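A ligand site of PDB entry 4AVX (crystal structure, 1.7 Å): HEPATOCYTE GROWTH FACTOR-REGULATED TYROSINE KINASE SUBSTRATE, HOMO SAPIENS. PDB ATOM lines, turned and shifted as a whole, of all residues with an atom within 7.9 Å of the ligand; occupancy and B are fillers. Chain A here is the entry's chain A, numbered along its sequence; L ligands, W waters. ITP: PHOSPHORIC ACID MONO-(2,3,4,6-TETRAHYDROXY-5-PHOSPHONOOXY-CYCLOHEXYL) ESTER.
N of His 182 is in hydrogen-bond range of O11 of the ligand (3.0 Å).
NE of Arg 211 lies within salt-bridge range of O10 of the ligand.
An oxygen (O4) of the ligand sits at hydrogen-bond distance from a ring nitrogen (ND1) of His 182, 2.8 Å away.
OP3 of the ligand lies within salt-bridge range of NE of Arg 179 (2.8 Å).
ND1 of His 181 is in hydrogen-bond range of O10 of the ligand (2.7 Å).
An oxygen (O11) of the ligand is in salt-bridge range of the guanidinium group of Arg 184, 2.8 Å away.
O of Ser 195 sits at hydrogen-bond distance from NH1 of Arg 211 (2.7 Å).
O of His 182 lies within hydrogen-bond range of NH1 of Arg 184 (2.8 Å).
The backbone NH (N) of Phe 190 sits at hydrogen-bond distance from the backbone carbonyl oxygen (O) of His 181 (2.8 Å).
The guanidinium group (NH2) of Arg 211 sits close to a ring nitrogen (ND1) of His 181 (3.4 Å).
The backbone NH (N) of Arg 184 is in hydrogen-bond range of the backbone carbonyl oxygen (O) of Arg 211, 2.9 Å away.
A ring nitrogen (NE2) of His 182 lies within hydrogen-bond range of the backbone carbonyl oxygen of Val 162 (2.6 Å).
OH of Tyr 198 sits at hydrogen-bond distance from NH2 of Arg 211, 3.3 Å away.
The side-chain amino group of Lys 180 is in salt-bridge range of the side-chain carboxylate of Asp 163 (2.8 Å).
Merely in contact with the ligand: Trp 161 and Lys 180.
Hydrophobic or aromatic side chains that line the ligand: Trp 161, His 181 and His 182.
Of the 19 residues printed, 7 come within 4 Å of the ligand.
Water W6 lies within hydrogen-bond range of the backbone carbonyl oxygen (O) of Lys 180 (2.7 Å) and an oxygen (OP3) of the ligand (2.8 Å).
Water W5 bridges O12 of the ligand (2.8 Å) and NE of Arg 211 (3.1 Å).
Water W3 bridges an oxygen (OP3) of the ligand and the backbone NH (N) of Lys 180.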
ATOM      1  N   TRP A 161      -6.024  30.197  -9.892  1.00  0.00           N
ATOM      2  CA  TRP A 161      -5.486  30.556  -8.634  1.00  0.00           C
ATOM      3  C   TRP A 161      -4.755  31.867  -8.654  1.00  0.00           C
ATOM      4  O   TRP A 161      -4.038  32.176  -9.596  1.00  0.00           O
ATOM      5  CB  TRP A 161      -4.602  29.459  -8.111  1.00  0.00           C
ATOM      6  CG  TRP A 161      -5.342  28.223  -7.751  1.00  0.00           C
ATOM      7  CD1 TRP A 161      -6.719  27.907  -7.925  1.00  0.00           C
ATOM      8  CD2 TRP A 161      -4.793  27.095  -7.038  1.00  0.00           C
ATOM      9  NE1 TRP A 161      -6.993  26.703  -7.408  1.00  0.00           N
ATOM     10  CE2 TRP A 161      -5.877  26.129  -6.906  1.00  0.00           C
ATOM     11  CE3 TRP A 161      -3.518  26.770  -6.571  1.00  0.00           C
ATOM     12  CZ2 TRP A 161      -5.681  24.902  -6.310  1.00  0.00           C
ATOM     13  CZ3 TRP A 161      -3.343  25.537  -5.970  1.00  0.00           C
ATOM     14  CH2 TRP A 161      -4.412  24.631  -5.822  1.00  0.00           C
ATOM     15  N   VAL A 162      -4.953  32.647  -7.617  1.00  0.00           N
ATOM     16  CA  VAL A 162      -4.300  33.961  -7.438  1.00  0.00           C
ATOM     17  C   VAL A 162      -2.980  33.831  -6.683  1.00  0.00           C
ATOM     18  O   VAL A 162      -2.891  33.069  -5.727  1.00  0.00           O
ATOM     19  CB  VAL A 162      -5.244  34.898  -6.646  1.00  0.00           C
ATOM     20  CG1 VAL A 162      -4.584  36.214  -6.227  1.00  0.00           C
ATOM     21  CG2 VAL A 162      -6.528  35.137  -7.440  1.00  0.00           C
ATOM     22  N   ASP A 163      -1.950  34.561  -7.092  1.00  0.00           N
ATOM     23  CA  ASP A 163      -0.746  34.700  -6.228  1.00  0.00           C
ATOM     24  C   ASP A 163      -0.660  36.052  -5.538  1.00  0.00           C
ATOM     25  O   ASP A 163      -0.982  37.084  -6.152  1.00  0.00           O
ATOM     26  CB  ASP A 163       0.546  34.442  -6.993  1.00  0.00           C
ATOM     27  CG  ASP A 163       1.773  34.312  -6.062  1.00  0.00           C
ATOM     28  OD1 ASP A 163       1.634  33.690  -4.966  1.00  0.00           O
ATOM     29  OD2 ASP A 163       2.872  34.824  -6.398  1.00  0.00           O
ATOM     30  N   GLY A 175       5.748  33.405   4.112  1.00  0.00           N
ATOM     31  CA  GLY A 175       7.195  33.232   4.238  1.00  0.00           C
ATOM     32  C   GLY A 175       7.507  31.754   4.242  1.00  0.00           C
ATOM     33  O   GLY A 175       6.597  30.924   4.018  1.00  0.00           O
ATOM     34  N   VAL A 176       8.773  31.408   4.524  1.00  0.00           N
ATOM     35  CA  VAL A 176       9.182  30.019   4.555  1.00  0.00           C
ATOM     36  C   VAL A 176       8.335  29.239   5.581  1.00  0.00           C
ATOM     37  O   VAL A 176       7.937  28.113   5.305  1.00  0.00           O
ATOM     38  CB  VAL A 176      10.699  29.833   4.875  1.00  0.00           C
ATOM     39  CG1 VAL A 176      11.052  28.370   4.885  1.00  0.00           C
ATOM     40  CG2 VAL A 176      11.560  30.559   3.824  1.00  0.00           C
ATOM     41  N   THR A 178       5.323  30.414   6.837  1.00  0.00           N
ATOM     42  CA  THR A 178       3.890  30.749   6.746  1.00  0.00           C
ATOM     43  C   THR A 178       3.537  30.484   5.332  1.00  0.00           C
ATOM     44  O   THR A 178       3.667  31.380   4.479  1.00  0.00           O
ATOM     45  CB  THR A 178       3.593  32.221   7.171  1.00  0.00           C
ATOM     46  OG1 THR A 178       4.015  32.418   8.518  1.00  0.00           O
ATOM     47  CG2 THR A 178       2.080  32.583   7.058  1.00  0.00           C
ATOM     48  N   ARG A 179       3.099  29.257   5.046  1.00  0.00           N
ATOM     49  CA  ARG A 179       3.068  28.781   3.638  1.00  0.00           C
ATOM     50  C   ARG A 179       1.714  29.036   2.995  1.00  0.00           C
ATOM     51  O   ARG A 179       0.729  29.349   3.677  1.00  0.00           O
ATOM     52  CB  ARG A 179       3.476  27.315   3.546  1.00  0.00           C
ATOM     53  CG  ARG A 179       4.874  27.097   4.156  1.00  0.00           C
ATOM     54  CD  ARG A 179       5.575  25.843   3.698  1.00  0.00           C
ATOM     55  NE  ARG A 179       5.999  25.930   2.316  1.00  0.00           N
ATOM     56  CZ  ARG A 179       7.180  26.333   1.885  1.00  0.00           C
ATOM     57  NH1 ARG A 179       8.121  26.766   2.729  1.00  0.00           N
ATOM     58  NH2 ARG A 179       7.448  26.284   0.580  1.00  0.00           N
ATOM     59  N   LYS A 180       1.750  29.021   1.654  1.00  0.00           N
ATOM     60  CA  LYS A 180       0.575  29.338   0.831  1.00  0.00           C
ATOM     61  C   LYS A 180      -0.320  28.162   0.598  1.00  0.00           C
ATOM     62  O   LYS A 180       0.096  27.038   0.401  1.00  0.00           O
ATOM     63  CB  LYS A 180       1.035  29.898  -0.499  1.00  0.00           C
ATOM     64  CG  LYS A 180       1.761  31.182  -0.370  1.00  0.00           C
ATOM     65  CD  LYS A 180       2.495  31.485  -1.667  1.00  0.00           C
ATOM     66  CE  LYS A 180       3.055  32.888  -1.618  1.00  0.00           C
ATOM     67  NZ  LYS A 180       3.605  33.214  -2.971  1.00  0.00           N
ATOM     68  N   HIS A 181      -1.618  28.464   0.578  1.00  0.00           N
ATOM     69  CA  HIS A 181      -2.650  27.510   0.197  1.00  0.00           C
ATOM     70  C   HIS A 181      -3.671  28.229  -0.656  1.00  0.00           C
ATOM     71  O   HIS A 181      -3.776  29.454  -0.661  1.00  0.00           O
ATOM     72  CB  HIS A 181      -3.343  26.956   1.453  1.00  0.00           C
ATOM     73  CG  HIS A 181      -2.398  26.320   2.417  1.00  0.00           C
ATOM     74  ND1 HIS A 181      -1.925  25.024   2.268  1.00  0.00           N
ATOM     75  CD2 HIS A 181      -1.723  26.862   3.521  1.00  0.00           C
ATOM     76  CE1 HIS A 181      -1.020  24.777   3.251  1.00  0.00           C
ATOM     77  NE2 HIS A 181      -0.924  25.886   4.038  1.00  0.00           N
ATOM     78  N   HIS A 182      -4.506  27.472  -1.367  1.00  0.00           N
ATOM     79  CA  HIS A 182      -5.561  28.082  -2.140  1.00  0.00           C
ATOM     80  C   HIS A 182      -6.891  27.473  -1.897  1.00  0.00           C
ATOM     81  O   HIS A 182      -6.982  26.229  -1.708  1.00  0.00           O
ATOM     82  CB  HIS A 182      -5.238  27.925  -3.624  1.00  0.00           C
ATOM     83  CG  HIS A 182      -4.167  28.898  -4.086  1.00  0.00           C
ATOM     84  ND1 HIS A 182      -2.822  28.615  -4.031  1.00  0.00           N
ATOM     85  CD2 HIS A 182      -4.290  30.187  -4.594  1.00  0.00           C
ATOM     86  CE1 HIS A 182      -2.136  29.683  -4.467  1.00  0.00           C
ATOM     87  NE2 HIS A 182      -3.022  30.650  -4.818  1.00  0.00           N
ATOM     88  N   CYS A 183      -7.908  28.309  -1.995  1.00  0.00           N
ATOM     89  CA  CYS A 183      -9.297  27.850  -1.989  1.00  0.00           C
ATOM     90  C   CYS A 183      -9.696  27.450  -3.396  1.00  0.00           C
ATOM     91  O   CYS A 183      -9.566  28.270  -4.330  1.00  0.00           O
ATOM     92  CB  CYS A 183     -10.221  28.928  -1.440  1.00  0.00           C
ATOM     93  SG  CYS A 183     -11.955  28.508  -1.678  1.00  0.00           S
ATOM     94  N   ARG A 184     -10.131  26.195  -3.595  1.00  0.00           N
ATOM     95  CA  ARG A 184     -10.504  25.682  -4.901  1.00  0.00           C
ATOM     96  C   ARG A 184     -11.791  26.344  -5.410  1.00  0.00           C
ATOM     97  O   ARG A 184     -12.005  26.417  -6.658  1.00  0.00           O
ATOM     98  CB  ARG A 184     -10.654  24.144  -4.910  1.00  0.00           C
ATOM     99  CG  ARG A 184      -9.361  23.394  -5.107  1.00  0.00           C
ATOM    100  CD  ARG A 184      -8.388  23.612  -3.941  1.00  0.00           C
ATOM    101  NE  ARG A 184      -7.290  22.665  -4.037  1.00  0.00           N
ATOM    102  CZ  ARG A 184      -6.120  22.823  -3.424  1.00  0.00           C
ATOM    103  NH1 ARG A 184      -5.860  23.911  -2.712  1.00  0.00           N
ATOM    104  NH2 ARG A 184      -5.200  21.887  -3.562  1.00  0.00           N
ATOM    105  N   GLN A 188      -8.671  32.203  -4.359  1.00  0.00           N
ATOM    106  CA  GLN A 188      -7.842  33.103  -3.607  1.00  0.00           C
ATOM    107  C   GLN A 188      -6.803  32.349  -2.794  1.00  0.00           C
ATOM    108  O   GLN A 188      -6.895  31.153  -2.577  1.00  0.00           O
ATOM    109  CB  GLN A 188      -8.697  33.973  -2.735  1.00  0.00           C
ATOM    110  CG  GLN A 188      -9.051  35.246  -3.464  1.00  0.00           C
ATOM    111  CD  GLN A 188      -7.871  36.231  -3.559  1.00  0.00           C
ATOM    112  OE1 GLN A 188      -6.667  35.939  -3.212  1.00  0.00           O
ATOM    113  NE2 GLN A 188      -8.182  37.392  -4.081  1.00  0.00           N
ATOM    114  N   ILE A 189      -5.814  33.111  -2.315  1.00  0.00           N
ATOM    115  CA  ILE A 189      -4.665  32.560  -1.610  1.00  0.00           C
ATOM    116  C   ILE A 189      -4.771  32.850  -0.122  1.00  0.00           C
ATOM    117  O   ILE A 189      -5.220  33.945   0.295  1.00  0.00           O
ATOM    118  CB  ILE A 189      -3.333  33.119  -2.226  1.00  0.00           C
ATOM    119  CG1 ILE A 189      -2.123  32.275  -1.793  1.00  0.00           C
ATOM    120  CG2 ILE A 189      -3.158  34.599  -1.896  1.00  0.00           C
ATOM    121  CD1 ILE A 189      -0.852  32.630  -2.568  1.00  0.00           C
ATOM    122  N   PHE A 190      -4.500  31.833   0.674  1.00  0.00           N
ATOM    123  CA  PHE A 190      -4.738  31.863   2.089  1.00  0.00           C
ATOM    124  C   PHE A 190      -3.636  31.213   2.889  1.00  0.00           C
ATOM    125  O   PHE A 190      -2.981  30.271   2.415  1.00  0.00           O
ATOM    126  CB  PHE A 190      -6.052  31.144   2.456  1.00  0.00           C
ATOM    127  CG  PHE A 190      -7.276  31.746   1.850  1.00  0.00           C
ATOM    128  CD1 PHE A 190      -7.741  31.342   0.585  1.00  0.00           C
ATOM    129  CD2 PHE A 190      -7.987  32.740   2.512  1.00  0.00           C
ATOM    130  CE1 PHE A 190      -8.858  31.931   0.040  1.00  0.00           C
ATOM    131  CE2 PHE A 190      -9.074  33.345   1.936  1.00  0.00           C
ATOM    132  CZ  PHE A 190      -9.529  32.911   0.712  1.00  0.00           C
ATOM    133  N   GLY A 192      -2.920  28.642   6.115  1.00  0.00           N
ATOM    134  CA  GLY A 192      -3.552  27.392   6.536  1.00  0.00           C
ATOM    135  C   GLY A 192      -4.721  27.583   7.478  1.00  0.00           C
ATOM    136  O   GLY A 192      -5.775  26.965   7.271  1.00  0.00           O
ATOM    137  N   SER A 195      -7.860  28.567   5.560  1.00  0.00           N
ATOM    138  CA  SER A 195      -8.286  27.613   4.496  1.00  0.00           C
ATOM    139  C   SER A 195      -8.228  26.164   4.983  1.00  0.00           C
ATOM    140  O   SER A 195      -7.693  25.294   4.320  1.00  0.00           O
ATOM    141  CB  SER A 195      -7.460  27.799   3.234  1.00  0.00           C
ATOM    142  OG  SER A 195      -6.084  27.586   3.461  1.00  0.00           O
ATOM    143  N   TYR A 198     -12.842  21.696   4.052  1.00  0.00           N
ATOM    144  CA  TYR A 198     -12.825  20.845   2.904  1.00  0.00           C
ATOM    145  C   TYR A 198     -14.264  20.641   2.475  1.00  0.00           C
ATOM    146  O   TYR A 198     -15.163  20.478   3.324  1.00  0.00           O
ATOM    147  CB  TYR A 198     -12.124  19.512   3.189  1.00  0.00           C
ATOM    148  CG  TYR A 198     -10.641  19.708   3.289  1.00  0.00           C
ATOM    149  CD1 TYR A 198     -10.046  20.123   4.495  1.00  0.00           C
ATOM    150  CD2 TYR A 198      -9.826  19.546   2.187  1.00  0.00           C
ATOM    151  CE1 TYR A 198      -8.679  20.338   4.573  1.00  0.00           C
ATOM    152  CE2 TYR A 198      -8.446  19.751   2.249  1.00  0.00           C
ATOM    153  CZ  TYR A 198      -7.888  20.160   3.454  1.00  0.00           C
ATOM    154  OH  TYR A 198      -6.524  20.364   3.510  1.00  0.00           O
ATOM    155  N   ARG A 211      -9.784  21.631  -0.560  1.00  0.00           N
ATOM    156  CA  ARG A 211      -9.572  22.741   0.339  1.00  0.00           C
ATOM    157  C   ARG A 211     -10.325  24.000  -0.097  1.00  0.00           C
ATOM    158  O   ARG A 211     -10.262  24.376  -1.311  1.00  0.00           O
ATOM    159  CB  ARG A 211      -8.066  23.080   0.353  1.00  0.00           C
ATOM    160  CG  ARG A 211      -7.721  24.213   1.274  1.00  0.00           C
ATOM    161  CD  ARG A 211      -6.281  24.640   1.299  1.00  0.00           C
ATOM    162  NE  ARG A 211      -5.373  23.583   1.759  1.00  0.00           N
ATOM    163  CZ  ARG A 211      -4.893  23.469   3.006  1.00  0.00           C
ATOM    164  NH1 ARG A 211      -5.191  24.349   3.939  1.00  0.00           N
ATOM    165  NH2 ARG A 211      -4.033  22.487   3.258  1.00  0.00           N
HETATM  166  C1  ITP L   1       2.088  25.397  -2.015  1.00  0.00           C
HETATM  167  O1  ITP L   1       3.454  24.908  -2.179  1.00  0.00           O
HETATM  168  C2  ITP L   1       1.102  24.187  -2.102  1.00  0.00           C
HETATM  169  O2  ITP L   1       1.260  23.387  -3.279  1.00  0.00           O
HETATM  170  C3  ITP L   1      -0.310  24.683  -2.036  1.00  0.00           C
HETATM  171  O3  ITP L   1      -1.146  23.652  -2.160  1.00  0.00           O
HETATM  172  C4  ITP L   1      -0.597  25.645  -3.100  1.00  0.00           C
HETATM  173  O4  ITP L   1      -1.930  26.204  -2.934  1.00  0.00           O
HETATM  174  C5  ITP L   1       0.364  26.854  -3.014  1.00  0.00           C
HETATM  175  O5  ITP L   1       0.123  27.736  -4.086  1.00  0.00           O
HETATM  176  C6  ITP L   1       1.811  26.428  -3.095  1.00  0.00           C
HETATM  177  O6  ITP L   1       2.672  27.575  -2.912  1.00  0.00           O
HETATM  178  P1  ITP L   1       4.371  24.611  -0.877  1.00  0.00           P
HETATM  179  OP1 ITP L   1       5.818  24.854  -1.443  1.00  0.00           O
HETATM  180  OP2 ITP L   1       4.204  23.109  -0.518  1.00  0.00           O
HETATM  181  OP3 ITP L   1       4.073  25.516   0.263  1.00  0.00           O
HETATM  182  P3  ITP L   1      -2.471  23.457  -1.231  1.00  0.00           P
HETATM  183  O10 ITP L   1      -2.126  23.291   0.267  1.00  0.00           O
HETATM  184  O11 ITP L   1      -3.425  24.660  -1.541  1.00  0.00           O
HETATM  185  O12 ITP L   1      -3.062  22.117  -1.707  1.00  0.00           O
HETATM  186  O   HOH W   1       3.491  22.538  -4.715  1.00  0.00           O
HETATM  187  O   HOH W   2       0.321  22.462   1.141  1.00  0.00           O
HETATM  188  O   HOH W   3       4.139  28.324   0.197  1.00  0.00           O
HETATM  189  O   HOH W   4       4.316  22.578   2.107  1.00  0.00           O
HETATM  190  O   HOH W   5      -5.118  21.147  -0.122  1.00  0.00           O
HETATM  191  O   HOH W   6       1.648  25.113   1.509  1.00  0.00           O
HETATM  192  O   HOH W   7       5.457  27.237  -2.996  1.00  0.00           O
HETATM  193  O   HOH W   8      -1.728  21.798  -4.838  1.00  0.00           O
HETATM  194  O   HOH W   9      -1.929  20.015  -2.329  1.00  0.00           O
